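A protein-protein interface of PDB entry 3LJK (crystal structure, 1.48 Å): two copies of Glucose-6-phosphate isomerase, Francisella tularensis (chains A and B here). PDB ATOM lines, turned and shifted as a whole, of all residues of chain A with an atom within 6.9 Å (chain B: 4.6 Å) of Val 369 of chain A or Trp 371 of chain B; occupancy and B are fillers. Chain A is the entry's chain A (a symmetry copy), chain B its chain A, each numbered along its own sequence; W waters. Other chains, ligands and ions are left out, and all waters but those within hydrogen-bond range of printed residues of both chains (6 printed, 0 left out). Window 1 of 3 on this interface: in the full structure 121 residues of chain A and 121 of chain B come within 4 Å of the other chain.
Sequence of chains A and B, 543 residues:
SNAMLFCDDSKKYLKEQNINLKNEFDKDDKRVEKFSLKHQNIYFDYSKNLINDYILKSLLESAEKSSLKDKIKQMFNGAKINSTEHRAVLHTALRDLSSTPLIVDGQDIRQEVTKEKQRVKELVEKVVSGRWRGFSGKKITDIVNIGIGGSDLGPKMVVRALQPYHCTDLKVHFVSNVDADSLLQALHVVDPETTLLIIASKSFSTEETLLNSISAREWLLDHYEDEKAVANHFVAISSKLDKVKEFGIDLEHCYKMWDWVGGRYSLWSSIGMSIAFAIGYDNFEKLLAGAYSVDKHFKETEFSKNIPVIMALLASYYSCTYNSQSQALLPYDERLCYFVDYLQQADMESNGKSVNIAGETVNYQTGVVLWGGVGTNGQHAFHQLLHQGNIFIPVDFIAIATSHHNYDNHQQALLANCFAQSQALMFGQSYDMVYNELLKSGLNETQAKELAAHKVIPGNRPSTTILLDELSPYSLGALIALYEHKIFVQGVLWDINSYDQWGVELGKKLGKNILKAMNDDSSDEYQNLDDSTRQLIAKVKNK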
ATOM      1  N   GLN A 325       1.161 -22.945  22.051  1.00  0.00           N
ATOM      2  CA  GLN A 325       1.520 -21.859  21.154  1.00  0.00           C
ATOM      3  C   GLN A 325       3.021 -21.831  20.853  1.00  0.00           C
ATOM      4  O   GLN A 325       3.513 -20.877  20.241  1.00  0.00           O
ATOM      5  CB  GLN A 325       1.057 -20.491  21.680  1.00  0.00           C
ATOM      6  CG  GLN A 325      -0.465 -20.412  21.913  1.00  0.00           C
ATOM      7  CD  GLN A 325      -0.937 -19.099  22.517  1.00  0.00           C
ATOM      8  OE1 GLN A 325      -0.202 -18.139  22.539  1.00  0.00           O
ATOM      9  NE2 GLN A 325      -2.066 -19.131  23.187  1.00  0.00           N
ATOM     10  N   SER A 326       3.751 -22.877  21.253  1.00  0.00           N
ATOM     11  CA  SER A 326       5.167 -23.013  20.922  1.00  0.00           C
ATOM     12  C   SER A 326       5.561 -24.477  20.951  1.00  0.00           C
ATOM     13  O   SER A 326       4.836 -25.329  21.480  1.00  0.00           O
ATOM     14  CB  SER A 326       6.085 -22.207  21.875  1.00  0.00           C
ATOM     15  OG  SER A 326       6.300 -22.864  23.110  1.00  0.00           O
ATOM     16  N   GLN A 327       6.724 -24.735  20.360  1.00  0.00           N
ATOM     17  CA  GLN A 327       7.374 -26.040  20.371  1.00  0.00           C
ATOM     18  C   GLN A 327       8.835 -25.800  20.652  1.00  0.00           C
ATOM     19  O   GLN A 327       9.423 -24.849  20.113  1.00  0.00           O
ATOM     20  CB  GLN A 327       7.310 -26.711  18.953  1.00  0.00           C
ATOM     21  CG  GLN A 327       5.961 -27.244  18.566  1.00  0.00           C
ATOM     22  CD  GLN A 327       5.980 -27.784  17.147  1.00  0.00           C
ATOM     23  OE1 GLN A 327       6.122 -28.995  16.957  1.00  0.00           O
ATOM     24  NE2 GLN A 327       5.946 -26.890  16.169  1.00  0.00           N
ATOM     25  N   ALA A 328       9.447 -26.656  21.480  1.00  0.00           N
ATOM     26  CA  ALA A 328      10.871 -26.589  21.800  1.00  0.00           C
ATOM     27  C   ALA A 328      11.666 -27.668  21.052  1.00  0.00           C
ATOM     28  O   ALA A 328      11.250 -28.817  20.991  1.00  0.00           O
ATOM     29  CB  ALA A 328      11.082 -26.779  23.327  1.00  0.00           C
ATOM     30  N   GLN A 344      13.489 -22.005  12.597  1.00  0.00           N
ATOM     31  CA  GLN A 344      12.546 -20.912  12.860  1.00  0.00           C
ATOM     32  C   GLN A 344      12.097 -20.288  11.560  1.00  0.00           C
ATOM     33  O   GLN A 344      10.906 -20.033  11.373  1.00  0.00           O
ATOM     34  CB  GLN A 344      13.136 -19.812  13.727  1.00  0.00           C
ATOM     35  CG  GLN A 344      13.237 -20.171  15.124  1.00  0.00           C
ATOM     36  CD  GLN A 344      13.795 -19.060  15.977  1.00  0.00           C
ATOM     37  OE1 GLN A 344      14.644 -18.252  15.522  1.00  0.00           O
ATOM     38  NE2 GLN A 344      13.322 -18.993  17.234  1.00  0.00           N
ATOM     39  N   ASP A 347      10.022 -23.044   9.385  1.00  0.00           N
ATOM     40  CA  ASP A 347       8.713 -23.350   9.985  1.00  0.00           C
ATOM     41  C   ASP A 347       7.828 -22.112  10.049  1.00  0.00           C
ATOM     42  O   ASP A 347       6.778 -22.036   9.394  1.00  0.00           O
ATOM     43  CB  ASP A 347       8.964 -23.960  11.356  1.00  0.00           C
ATOM     44  CG  ASP A 347       7.749 -24.495  12.044  1.00  0.00           C
ATOM     45  OD1 ASP A 347       6.627 -24.242  11.573  1.00  0.00           O
ATOM     46  OD2 ASP A 347       7.932 -25.204  13.081  1.00  0.00           O
ATOM     47  N   MET A 348       8.286 -21.074  10.732  1.00  0.00           N
ATOM     48  CA  MET A 348       7.421 -19.921  11.034  1.00  0.00           C
ATOM     49  C   MET A 348       7.123 -19.084   9.814  1.00  0.00           C
ATOM     50  O   MET A 348       6.012 -18.580   9.684  1.00  0.00           O
ATOM     51  CB  MET A 348       7.976 -19.053  12.158  1.00  0.00           C
ATOM     52  CG  MET A 348       8.184 -19.858  13.442  1.00  0.00           C
ATOM     53  SD  MET A 348       9.145 -18.898  14.857  1.00  0.00           S
ATOM     54  CE  MET A 348       8.062 -18.030  15.143  1.00  0.00           C
ATOM     55  N   THR A 366      -2.842 -21.686  13.409  1.00  0.00           N
ATOM     56  CA  THR A 366      -1.935 -22.296  12.437  1.00  0.00           C
ATOM     57  C   THR A 366      -0.523 -22.397  13.057  1.00  0.00           C
ATOM     58  O   THR A 366      -0.382 -22.873  14.197  1.00  0.00           O
ATOM     59  CB  THR A 366      -1.998 -21.560  11.095  1.00  0.00           C
ATOM     60  OG1 THR A 366      -1.654 -20.181  11.310  1.00  0.00           O
ATOM     61  CG2 THR A 366      -3.396 -21.720  10.472  1.00  0.00           C
ATOM     62  N   GLY A 367       0.532 -21.907  12.391  1.00  0.00           N
ATOM     63  CA  GLY A 367       1.880 -22.164  12.864  1.00  0.00           C
ATOM     64  C   GLY A 367       2.170 -21.514  14.183  1.00  0.00           C
ATOM     65  O   GLY A 367       1.693 -20.418  14.450  1.00  0.00           O
ATOM     66  N   VAL A 368       2.921 -22.236  15.036  1.00  0.00           N
ATOM     67  CA  VAL A 368       3.290 -21.742  16.356  1.00  0.00           C
ATOM     68  C   VAL A 368       4.786 -21.319  16.381  1.00  0.00           C
ATOM     69  O   VAL A 368       5.556 -21.511  15.423  1.00  0.00           O
ATOM     70  CB  VAL A 368       2.941 -22.766  17.447  1.00  0.00           C
ATOM     71  CG1 VAL A 368       1.435 -23.132  17.373  1.00  0.00           C
ATOM     72  CG2 VAL A 368       3.826 -24.021  17.457  1.00  0.00           C
ATOM     73  N   VAL A 369       5.180 -20.772  17.538  1.00  0.00           N
ATOM     74  CA  VAL A 369       6.562 -20.362  17.744  1.00  0.00           C
ATOM     75  C   VAL A 369       7.456 -21.591  17.883  1.00  0.00           C
ATOM     76  O   VAL A 369       7.169 -22.482  18.690  1.00  0.00           O
ATOM     77  CB  VAL A 369       6.673 -19.447  18.978  1.00  0.00           C
ATOM     78  CG1 VAL A 369       8.138 -19.113  19.275  1.00  0.00           C
ATOM     79  CG2 VAL A 369       5.833 -18.181  18.766  1.00  0.00           C
ATOM     80  N   LEU A 370       8.558 -21.619  17.147  1.00  0.00           N
ATOM     81  CA  LEU A 370       9.583 -22.617  17.285  1.00  0.00           C
ATOM     82  C   LEU A 370      10.742 -21.983  18.023  1.00  0.00           C
ATOM     83  O   LEU A 370      11.202 -20.920  17.595  1.00  0.00           O
ATOM     84  CB  LEU A 370      10.046 -23.169  15.926  1.00  0.00           C
ATOM     85  CG  LEU A 370      10.976 -24.388  15.970  1.00  0.00           C
ATOM     86  CD1 LEU A 370      10.430 -25.592  16.686  1.00  0.00           C
ATOM     87  CD2 LEU A 370      11.424 -24.751  14.565  1.00  0.00           C
ATOM     88  N   TRP A 371      11.223 -22.626  19.080  1.00  0.00           N
ATOM     89  CA  TRP A 371      12.356 -22.093  19.821  1.00  0.00           C
ATOM     90  C   TRP A 371      13.122 -23.273  20.401  1.00  0.00           C
ATOM     91  O   TRP A 371      12.711 -24.431  20.244  1.00  0.00           O
ATOM     92  CB  TRP A 371      11.874 -21.094  20.947  1.00  0.00           C
ATOM     93  CG  TRP A 371      11.053 -21.784  22.007  1.00  0.00           C
ATOM     94  CD1 TRP A 371       9.761 -22.189  21.897  1.00  0.00           C
ATOM     95  CD2 TRP A 371      11.512 -22.246  23.271  1.00  0.00           C
ATOM     96  NE1 TRP A 371       9.354 -22.853  23.032  1.00  0.00           N
ATOM     97  CE2 TRP A 371      10.428 -22.921  23.894  1.00  0.00           C
ATOM     98  CE3 TRP A 371      12.715 -22.136  23.956  1.00  0.00           C
ATOM     99  CZ2 TRP A 371      10.531 -23.485  25.192  1.00  0.00           C
ATOM    100  CZ3 TRP A 371      12.815 -22.732  25.219  1.00  0.00           C
ATOM    101  CH2 TRP A 371      11.741 -23.368  25.827  1.00  0.00           C
ATOM    102  N   GLY A 372      14.223 -23.001  21.112  1.00  0.00           N
ATOM    103  CA  GLY A 372      14.929 -24.042  21.824  1.00  0.00           C
ATOM    104  C   GLY A 372      16.346 -23.688  22.091  1.00  0.00           C
ATOM    105  O   GLY A 372      16.662 -22.518  22.307  1.00  0.00           O
ATOM    106  N   SER B 326       4.087 -16.696  24.973  1.00  0.00           N
ATOM    107  CA  SER B 326       5.459 -16.316  24.646  1.00  0.00           C
ATOM    108  C   SER B 326       5.551 -14.809  24.503  1.00  0.00           C
ATOM    109  O   SER B 326       4.538 -14.109  24.383  1.00  0.00           O
ATOM    110  CB  SER B 326       5.977 -16.996  23.355  1.00  0.00           C
ATOM    111  OG  SER B 326       5.510 -16.361  22.180  1.00  0.00           O
ATOM    112  N   GLN B 327       6.796 -14.341  24.526  1.00  0.00           N
ATOM    113  CA  GLN B 327       7.148 -12.947  24.279  1.00  0.00           C
ATOM    114  C   GLN B 327       8.351 -12.954  23.369  1.00  0.00           C
ATOM    115  O   GLN B 327       9.264 -13.774  23.554  1.00  0.00           O
ATOM    116  CB  GLN B 327       7.611 -12.242  25.602  1.00  0.00           C
ATOM    117  CG  GLN B 327       6.506 -11.924  26.568  1.00  0.00           C
ATOM    118  CD  GLN B 327       7.063 -11.333  27.851  1.00  0.00           C
ATOM    119  OE1 GLN B 327       7.072 -10.109  28.005  1.00  0.00           O
ATOM    120  NE2 GLN B 327       7.615 -12.182  28.707  1.00  0.00           N
ATOM    121  N   ALA B 328       8.381 -12.042  22.390  1.00  0.00           N
ATOM    122  CA  ALA B 328       9.504 -11.886  21.469  1.00  0.00           C
ATOM    123  C   ALA B 328      10.358 -10.662  21.828  1.00  0.00           C
ATOM    124  O   ALA B 328       9.830  -9.595  22.112  1.00  0.00           O
ATOM    125  CB  ALA B 328       8.981 -11.723  20.015  1.00  0.00           C
ATOM    126  N   LEU B 329      11.663 -10.846  21.783  1.00  0.00           N
ATOM    127  CA  LEU B 329      12.620  -9.833  22.078  1.00  0.00           C
ATOM    128  C   LEU B 329      13.518  -9.733  20.838  1.00  0.00           C
ATOM    129  O   LEU B 329      14.179 -10.733  20.475  1.00  0.00           O
ATOM    130  CB  LEU B 329      13.398 -10.205  23.347  1.00  0.00           C
ATOM    131  CG  LEU B 329      14.583  -9.352  23.758  1.00  0.00           C
ATOM    132  CD1 LEU B 329      14.126  -7.949  24.026  1.00  0.00           C
ATOM    133  CD2 LEU B 329      15.238  -9.969  25.003  1.00  0.00           C
ATOM    134  N   VAL B 340      19.174 -12.517  23.892  1.00  0.00           N
ATOM    135  CA  VAL B 340      18.010 -13.362  24.069  1.00  0.00           C
ATOM    136  C   VAL B 340      18.361 -14.638  24.836  1.00  0.00           C
ATOM    137  O   VAL B 340      17.659 -15.023  25.787  1.00  0.00           O
ATOM    138  CB  VAL B 340      17.282 -13.668  22.729  1.00  0.00           C
ATOM    139  CG1 VAL B 340      16.235 -14.791  22.941  1.00  0.00           C
ATOM    140  CG2 VAL B 340      16.639 -12.383  22.099  1.00  0.00           C
ATOM    141  N   GLN B 344      16.649 -15.614  28.370  1.00  0.00           N
ATOM    142  CA  GLN B 344      15.882 -16.857  28.509  1.00  0.00           C
ATOM    143  C   GLN B 344      16.166 -17.495  29.848  1.00  0.00           C
ATOM    144  O   GLN B 344      15.242 -17.936  30.535  1.00  0.00           O
ATOM    145  CB  GLN B 344      16.197 -17.877  27.429  1.00  0.00           C
ATOM    146  CG  GLN B 344      15.608 -17.561  26.148  1.00  0.00           C
ATOM    147  CD  GLN B 344      15.905 -18.597  25.093  1.00  0.00           C
ATOM    148  OE1 GLN B 344      16.988 -19.236  25.092  1.00  0.00           O
ATOM    149  NE2 GLN B 344      14.942 -18.790  24.174  1.00  0.00           N
ATOM    150  N   VAL B 369       7.341 -18.390  27.584  1.00  0.00           N
ATOM    151  CA  VAL B 369       8.535 -18.574  26.770  1.00  0.00           C
ATOM    152  C   VAL B 369       9.057 -17.222  26.297  1.00  0.00           C
ATOM    153  O   VAL B 369       8.300 -16.422  25.737  1.00  0.00           O
ATOM    154  CB  VAL B 369       8.236 -19.507  25.580  1.00  0.00           C
ATOM    155  CG1 VAL B 369       9.450 -19.606  24.651  1.00  0.00           C
ATOM    156  CG2 VAL B 369       7.798 -20.885  26.093  1.00  0.00           C
ATOM    157  N   LEU B 370      10.350 -16.985  26.468  1.00  0.00           N
ATOM    158  CA  LEU B 370      11.027 -15.837  25.928  1.00  0.00           C
ATOM    159  C   LEU B 370      11.826 -16.299  24.729  1.00  0.00           C
ATOM    160  O   LEU B 370      12.596 -17.255  24.867  1.00  0.00           O
ATOM    161  CB  LEU B 370      11.947 -15.163  26.962  1.00  0.00           C
ATOM    162  CG  LEU B 370      12.546 -13.810  26.557  1.00  0.00           C
ATOM    163  CD1 LEU B 370      11.549 -12.742  26.205  1.00  0.00           C
ATOM    164  CD2 LEU B 370      13.505 -13.325  27.630  1.00  0.00           C
ATOM    165  N   TRP B 371      11.674 -15.628  23.594  1.00  0.00           N
ATOM    166  CA  TRP B 371      12.431 -15.995  22.407  1.00  0.00           C
ATOM    167  C   TRP B 371      12.655 -14.728  21.594  1.00  0.00           C
ATOM    168  O   TRP B 371      12.171 -13.649  21.961  1.00  0.00           O
ATOM    169  CB  TRP B 371      11.672 -17.102  21.574  1.00  0.00           C
ATOM    170  CG  TRP B 371      10.365 -16.598  21.016  1.00  0.00           C
ATOM    171  CD1 TRP B 371       9.210 -16.408  21.704  1.00  0.00           C
ATOM    172  CD2 TRP B 371      10.132 -16.117  19.699  1.00  0.00           C
ATOM    173  NE1 TRP B 371       8.237 -15.866  20.893  1.00  0.00           N
ATOM    174  CE2 TRP B 371       8.790 -15.655  19.649  1.00  0.00           C
ATOM    175  CE3 TRP B 371      10.906 -16.054  18.547  1.00  0.00           C
ATOM    176  CZ2 TRP B 371       8.212 -15.133  18.462  1.00  0.00           C
ATOM    177  CZ3 TRP B 371      10.336 -15.499  17.395  1.00  0.00           C
ATOM    178  CH2 TRP B 371       9.016 -15.073  17.352  1.00  0.00           C
ATOM    179  N   GLY B 372      13.354 -14.842  20.459  1.00  0.00           N
ATOM    180  CA  GLY B 372      13.489 -13.727  19.548  1.00  0.00           C
ATOM    181  C   GLY B 372      14.676 -13.853  18.667  1.00  0.00           C
ATOM    182  O   GLY B 372      15.052 -14.962  18.288  1.00  0.00           O
ATOM    183  N   PHE B 382      11.384 -14.894  10.797  1.00  0.00           N
ATOM    184  CA  PHE B 382      10.162 -15.152  11.540  1.00  0.00           C
ATOM    185  C   PHE B 382       9.194 -14.000  11.663  1.00  0.00           C
ATOM    186  O   PHE B 382       8.093 -14.185  12.206  1.00  0.00           O
ATOM    187  CB  PHE B 382      10.474 -15.754  12.917  1.00  0.00           C
ATOM    188  CG  PHE B 382      11.393 -14.916  13.743  1.00  0.00           C
ATOM    189  CD1 PHE B 382      10.910 -13.786  14.356  1.00  0.00           C
ATOM    190  CD2 PHE B 382      12.745 -15.219  13.831  1.00  0.00           C
ATOM    191  CE1 PHE B 382      11.760 -12.964  15.077  1.00  0.00           C
ATOM    192  CE2 PHE B 382      13.600 -14.385  14.555  1.00  0.00           C
ATOM    193  CZ  PHE B 382      13.093 -13.245  15.165  1.00  0.00           C
ATOM    194  N   LEU B 386       5.003 -12.944  12.985  1.00  0.00           N
ATOM    195  CA  LEU B 386       4.602 -11.804  13.806  1.00  0.00           C
ATOM    196  C   LEU B 386       3.555 -10.917  13.104  1.00  0.00           C
ATOM    197  O   LEU B 386       2.681 -10.343  13.773  1.00  0.00           O
ATOM    198  CB  LEU B 386       5.787 -10.959  14.239  1.00  0.00           C
ATOM    199  CG  LEU B 386       6.833 -11.640  15.123  1.00  0.00           C
ATOM    200  CD1 LEU B 386       8.014 -10.675  15.426  1.00  0.00           C
ATOM    201  CD2 LEU B 386       6.267 -12.244  16.415  1.00  0.00           C
ATOM    202  N   ILE B 393       1.514 -12.328  20.425  1.00  0.00           N
ATOM    203  CA  ILE B 393       2.869 -12.332  20.935  1.00  0.00           C
ATOM    204  C   ILE B 393       3.288 -10.861  21.190  1.00  0.00           C
ATOM    205  O   ILE B 393       3.487 -10.110  20.271  1.00  0.00           O
ATOM    206  CB  ILE B 393       3.860 -12.944  19.905  1.00  0.00           C
ATOM    207  CG1 ILE B 393       3.426 -14.352  19.510  1.00  0.00           C
ATOM    208  CG2 ILE B 393       5.283 -12.971  20.499  1.00  0.00           C
ATOM    209  CD1 ILE B 393       4.056 -14.907  18.225  1.00  0.00           C
HETATM  210  O   HOH W   1       1.714 -16.609  22.420  1.00  0.00           O
HETATM  211  O   HOH W   2      14.537 -17.409  19.398  1.00  0.00           O
HETATM  212  O   HOH W   3       3.714 -18.283  21.674  1.00  0.00           O
HETATM  213  O   HOH W   4      16.430 -16.814  16.690  1.00  0.00           O
HETATM  214  O   HOH W   5      18.280 -20.405  23.198  1.00  0.00           O
HETATM  215  O   HOH W   6      15.313 -20.235  21.637  1.00  0.00           O
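Asp 347 of chain A touches none of the printed residues of chain B.
Of the printed residues of chain B, Met 348 of chain A touches Trp 371 and Phe 382.
Val 368 of chain A touches none of the printed residues of chain B.
Val 369 of chain A touches just these residues of chain B: Ser 326 (3.9 Å), Trp 371 (3.5 Å) and Ile 393 (3.8 Å).
Of the printed residues of chain B, Trp 371 of chain A touches Val 369.
Printed residues of chain A within 4 Å of Phe 382 of chain B: Gln 344 and Met 348.
Printed residues of chain A within 4 Å of Ile 393 of chain B: Val 369.
The nearest printed residue of chain B that does not touch Val 369 of chain A is Val 369 of chain B (5.6 Å).
The nearest printed residue of chain A that does not touch Phe 382 of chain B is Leu 370 of chain A (7.0 Å).
NE1 of Trp 371 of chain A sits at hydrogen-bond distance from OG of Ser 326 of chain A (3.1 Å).
The side-chain amide nitrogen (NE2) of Gln 344 of chain A sits at hydrogen-bond distance from the backbone carbonyl oxygen (O) of Leu 370 of chain A, at 2.9 Å.
The backbone carbonyl oxygen (O) of Gln 325 of chain A lies within hydrogen-bond range of the backbone NH (N) of Val 369 of chain A, 3.2 Å away.
O of Trp 371 of chain B lies within hydrogen-bond range of N of Leu 329 of chain B (2.9 Å).
The backbone carbonyl oxygen (O) of Gln 327 of chain A is in hydrogen-bond range of the backbone NH (N) of Trp 371 of chain A, at 3.0 Å.
The backbone NH of Gln 327 of chain A sits at hydrogen-bond distance from the backbone carbonyl oxygen of Val 369 of chain A (2.8 Å).
Among the printed residues, merely in contact across the chains: Trp 371 of chain A with Val 369 of chain B (3.5 Å), Val 369 of chain A with Trp 371 of chain B (3.5 Å), Val 369 of chain A with Ile 393 of chain B (3.8 Å), Met 348 of chain A with Trp 371 of chain B (3.8 Å), Ser 326 of chain A with Val 369 of chain B (3.9 Å), Val 369 of chain A with Ser 326 of chain B (3.9 Å), Met 348 of chain A with Phe 382 of chain B (3.9 Å) and Gln 344 of chain A with Phe 382 of chain B (3.96 Å).
Water W1 lies within hydrogen-bond range of OE1 of Gln 325 of chain A and N of Ser 326 of chain B.
Water W4 lies within hydrogen-bond range of OE1 of Gln 344 of chain A (2.6 Å) and O of Gly 372 of chain B (2.8 Å).
Water W5 lies within hydrogen-bond range of OE1 of Gln 344 of chain B (2.6 Å) and O of Gly 372 of chain A (2.8 Å).
Water W3 bridges OG of Ser 326 of chain B (2.7 Å) and O of Gln 325 of chain A (3.0 Å).
Water W6 lies within hydrogen-bond range of O of Gly 372 of chain A (2.7 Å) and NE2 of Gln 344 of chain B (2.9 Å).
Water W2 lies within hydrogen-bond range of the backbone carbonyl oxygen (O) of Gly 372 of chain B (2.7 Å) and the side-chain amide nitrogen (NE2) of Gln 344 of chain A (2.9 Å).
Of the 14 printed residues of chain A, 5 touch a printed residue of chain B.
Along chain A the printed residues that touch a printed residue of chain B span positions 326 to 371.
Hydrophobic or aromatic side chains of chain B within 4 Å of the printed part of chain A: Val 369, Trp 371, Phe 382 and Ile 393.
Ser 326 of chain A touches Val 369 of chain B, and with the chains exchanged Val 369 of chain A touches Ser 326 of chain B.
Val 369 of chain A touches Trp 371 of chain B, and with the chains exchanged Trp 371 of chain A touches Val 369 of chain B.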
